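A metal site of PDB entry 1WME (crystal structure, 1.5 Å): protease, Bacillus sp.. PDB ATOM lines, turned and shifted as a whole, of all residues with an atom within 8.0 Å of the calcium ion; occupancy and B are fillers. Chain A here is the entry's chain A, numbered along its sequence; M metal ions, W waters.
The calcium ion is bound by OD1 of Asp 391 (2.2 Å), O of Thr 386 (2.4 Å), OD1 of Asp 384 (2.4 Å), water W1 (2.4 Å), O of Pro 388 (2.4 Å), OD1 of Asn 392 (2.5 Å), OD2 of Asp 384 (2.5 Å) and OG1 of Thr 386 (2.7 Å).
The calcium ion has eight donor atoms within binding distance.
Water W1 bridges the side-chain carboxylate of Asp 391 (2.7 Å) and the backbone carbonyl oxygen of Ser 387 (3.4 Å).
N of Asn 390 sits close to OD2 of Asp 384, 3.4 Å away.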
ATOM      1  N   VAL A 381     -16.318 -18.314  28.786  1.00  0.00           N
ATOM      2  CA  VAL A 381     -16.996 -17.929  30.036  1.00  0.00           C
ATOM      3  C   VAL A 381     -17.407 -16.473  29.975  1.00  0.00           C
ATOM      4  O   VAL A 381     -16.825 -15.654  29.268  1.00  0.00           O
ATOM      5  CB  VAL A 381     -16.152 -18.267  31.278  1.00  0.00           C
ATOM      6  CG1 VAL A 381     -15.648 -19.715  31.175  1.00  0.00           C
ATOM      7  CG2 VAL A 381     -14.995 -17.296  31.503  1.00  0.00           C
ATOM      8  N   ASN A 383     -18.085 -12.700  30.045  1.00  0.00           N
ATOM      9  CA  ASN A 383     -17.264 -11.489  30.076  1.00  0.00           C
ATOM     10  C   ASN A 383     -15.769 -11.752  29.914  1.00  0.00           C
ATOM     11  O   ASN A 383     -14.968 -10.819  30.163  1.00  0.00           O
ATOM     12  CB  ASN A 383     -17.506 -10.722  31.365  1.00  0.00           C
ATOM     13  CG  ASN A 383     -18.937 -10.200  31.421  1.00  0.00           C
ATOM     14  OD1 ASN A 383     -19.645 -10.170  30.405  1.00  0.00           O
ATOM     15  ND2 ASN A 383     -19.394  -9.761  32.584  1.00  0.00           N
ATOM     16  N   ASP A 384     -15.352 -12.941  29.437  1.00  0.00           N
ATOM     17  CA  ASP A 384     -13.917 -13.154  29.179  1.00  0.00           C
ATOM     18  C   ASP A 384     -13.673 -12.855  27.704  1.00  0.00           C
ATOM     19  O   ASP A 384     -14.040 -13.661  26.846  1.00  0.00           O
ATOM     20  CB  ASP A 384     -13.488 -14.601  29.506  1.00  0.00           C
ATOM     21  CG  ASP A 384     -12.008 -14.802  29.292  1.00  0.00           C
ATOM     22  OD1 ASP A 384     -11.304 -13.903  28.731  1.00  0.00           O
ATOM     23  OD2 ASP A 384     -11.453 -15.803  29.780  1.00  0.00           O
ATOM     24  N   PHE A 385     -13.095 -11.691  27.425  1.00  0.00           N
ATOM     25  CA  PHE A 385     -12.851 -11.266  26.061  1.00  0.00           C
ATOM     26  C   PHE A 385     -11.382 -11.395  25.642  1.00  0.00           C
ATOM     27  O   PHE A 385     -10.936 -10.796  24.649  1.00  0.00           O
ATOM     28  CB  PHE A 385     -13.317  -9.814  25.899  1.00  0.00           C
ATOM     29  CG  PHE A 385     -14.847  -9.745  25.952  1.00  0.00           C
ATOM     30  CD1 PHE A 385     -15.514  -9.448  27.130  1.00  0.00           C
ATOM     31  CD2 PHE A 385     -15.581  -9.964  24.793  1.00  0.00           C
ATOM     32  CE1 PHE A 385     -16.904  -9.359  27.140  1.00  0.00           C
ATOM     33  CE2 PHE A 385     -16.957  -9.898  24.780  1.00  0.00           C
ATOM     34  CZ  PHE A 385     -17.607  -9.602  25.965  1.00  0.00           C
ATOM     35  N   THR A 386     -10.604 -12.176  26.381  1.00  0.00           N
ATOM     36  CA  THR A 386      -9.208 -12.404  25.995  1.00  0.00           C
ATOM     37  C   THR A 386      -9.020 -13.896  25.828  1.00  0.00           C
ATOM     38  O   THR A 386      -9.402 -14.727  26.656  1.00  0.00           O
ATOM     39  CB  THR A 386      -8.189 -11.910  27.037  1.00  0.00           C
ATOM     40  OG1 THR A 386      -8.543 -12.487  28.329  1.00  0.00           O
ATOM     41  CG2 THR A 386      -8.239 -10.392  27.155  1.00  0.00           C
ATOM     42  N   SER A 387      -8.407 -14.290  24.730  1.00  0.00           N
ATOM     43  CA  SER A 387      -8.139 -15.695  24.491  1.00  0.00           C
ATOM     44  C   SER A 387      -7.038 -16.217  25.405  1.00  0.00           C
ATOM     45  O   SER A 387      -6.015 -15.532  25.624  1.00  0.00           O
ATOM     46  CB  SER A 387      -7.743 -15.851  23.001  1.00  0.00           C
ATOM     47  OG  SER A 387      -7.513 -17.211  22.720  1.00  0.00           O
ATOM     48  N   PRO A 388      -7.131 -17.418  25.949  1.00  0.00           N
ATOM     49  CA  PRO A 388      -8.301 -18.301  25.850  1.00  0.00           C
ATOM     50  C   PRO A 388      -9.482 -17.758  26.670  1.00  0.00           C
ATOM     51  O   PRO A 388      -9.269 -17.097  27.705  1.00  0.00           O
ATOM     52  CB  PRO A 388      -7.839 -19.616  26.464  1.00  0.00           C
ATOM     53  CG  PRO A 388      -6.607 -19.322  27.212  1.00  0.00           C
ATOM     54  CD  PRO A 388      -6.030 -18.042  26.705  1.00  0.00           C
ATOM     55  N   TYR A 389     -10.681 -18.047  26.178  1.00  0.00           N
ATOM     56  CA  TYR A 389     -11.889 -17.384  26.691  1.00  0.00           C
ATOM     57  C   TYR A 389     -12.523 -18.069  27.894  1.00  0.00           C
ATOM     58  O   TYR A 389     -13.684 -17.778  28.286  1.00  0.00           O
ATOM     59  CB  TYR A 389     -12.908 -17.334  25.552  1.00  0.00           C
ATOM     60  CG  TYR A 389     -12.342 -16.542  24.380  1.00  0.00           C
ATOM     61  CD1 TYR A 389     -12.053 -17.189  23.178  1.00  0.00           C
ATOM     62  CD2 TYR A 389     -12.088 -15.185  24.475  1.00  0.00           C
ATOM     63  CE1 TYR A 389     -11.539 -16.471  22.116  1.00  0.00           C
ATOM     64  CE2 TYR A 389     -11.556 -14.459  23.399  1.00  0.00           C
ATOM     65  CZ  TYR A 389     -11.290 -15.117  22.224  1.00  0.00           C
ATOM     66  OH  TYR A 389     -10.767 -14.425  21.152  1.00  0.00           O
ATOM     67  N   ASN A 390     -11.765 -18.964  28.527  1.00  0.00           N
ATOM     68  CA  ASN A 390     -12.316 -19.728  29.648  1.00  0.00           C
ATOM     69  C   ASN A 390     -11.451 -19.662  30.913  1.00  0.00           C
ATOM     70  O   ASN A 390     -11.622 -20.516  31.771  1.00  0.00           O
ATOM     71  CB  ASN A 390     -12.497 -21.199  29.249  1.00  0.00           C
ATOM     72  CG  ASN A 390     -11.182 -21.944  29.015  1.00  0.00           C
ATOM     73  OD1 ASN A 390     -10.186 -21.319  28.694  1.00  0.00           O
ATOM     74  ND2 ASN A 390     -11.150 -23.261  29.165  1.00  0.00           N
ATOM     75  N   ASP A 391     -10.567 -18.661  31.048  1.00  0.00           N
ATOM     76  CA  ASP A 391      -9.665 -18.550  32.174  1.00  0.00           C
ATOM     77  C   ASP A 391      -9.909 -17.296  33.016  1.00  0.00           C
ATOM     78  O   ASP A 391      -9.293 -17.211  34.079  1.00  0.00           O
ATOM     79  CB  ASP A 391      -8.185 -18.593  31.751  1.00  0.00           C
ATOM     80  CG  ASP A 391      -7.790 -17.525  30.769  1.00  0.00           C
ATOM     81  OD1 ASP A 391      -8.650 -16.632  30.454  1.00  0.00           O
ATOM     82  OD2 ASP A 391      -6.631 -17.522  30.286  1.00  0.00           O
ATOM     83  N   ASN A 392     -10.771 -16.388  32.596  1.00  0.00           N
ATOM     84  CA  ASN A 392     -11.065 -15.211  33.398  1.00  0.00           C
ATOM     85  C   ASN A 392     -12.535 -15.218  33.806  1.00  0.00           C
ATOM     86  O   ASN A 392     -13.393 -14.872  33.028  1.00  0.00           O
ATOM     87  CB  ASN A 392     -10.796 -13.892  32.648  1.00  0.00           C
ATOM     88  CG  ASN A 392      -9.349 -13.661  32.264  1.00  0.00           C
ATOM     89  OD1 ASN A 392      -8.972 -13.758  31.093  1.00  0.00           O
ATOM     90  ND2 ASN A 392      -8.491 -13.368  33.217  1.00  0.00           N
ATOM     91  N   TRP A 393     -12.848 -15.600  35.045  1.00  0.00           N
ATOM     92  CA  TRP A 393     -14.244 -15.702  35.442  1.00  0.00           C
ATOM     93  C   TRP A 393     -14.746 -14.431  36.071  1.00  0.00           C
ATOM     94  O   TRP A 393     -13.931 -13.724  36.697  1.00  0.00           O
ATOM     95  CB  TRP A 393     -14.384 -16.823  36.479  1.00  0.00           C
ATOM     96  CG  TRP A 393     -13.967 -18.151  35.920  1.00  0.00           C
ATOM     97  CD1 TRP A 393     -12.710 -18.627  35.691  1.00  0.00           C
ATOM     98  CD2 TRP A 393     -14.885 -19.161  35.513  1.00  0.00           C
ATOM     99  NE1 TRP A 393     -12.809 -19.893  35.165  1.00  0.00           N
ATOM    100  CE2 TRP A 393     -14.127 -20.241  35.048  1.00  0.00           C
ATOM    101  CE3 TRP A 393     -16.281 -19.236  35.520  1.00  0.00           C
ATOM    102  CZ2 TRP A 393     -14.719 -21.420  34.577  1.00  0.00           C
ATOM    103  CZ3 TRP A 393     -16.871 -20.401  35.046  1.00  0.00           C
ATOM    104  CH2 TRP A 393     -16.079 -21.468  34.589  1.00  0.00           C
HETATM  105 CA    CA M   1      -9.222 -15.031  29.003  1.00  0.00          CA
HETATM  106  O   HOH W   1      -6.803 -15.178  28.927  1.00  0.00           O
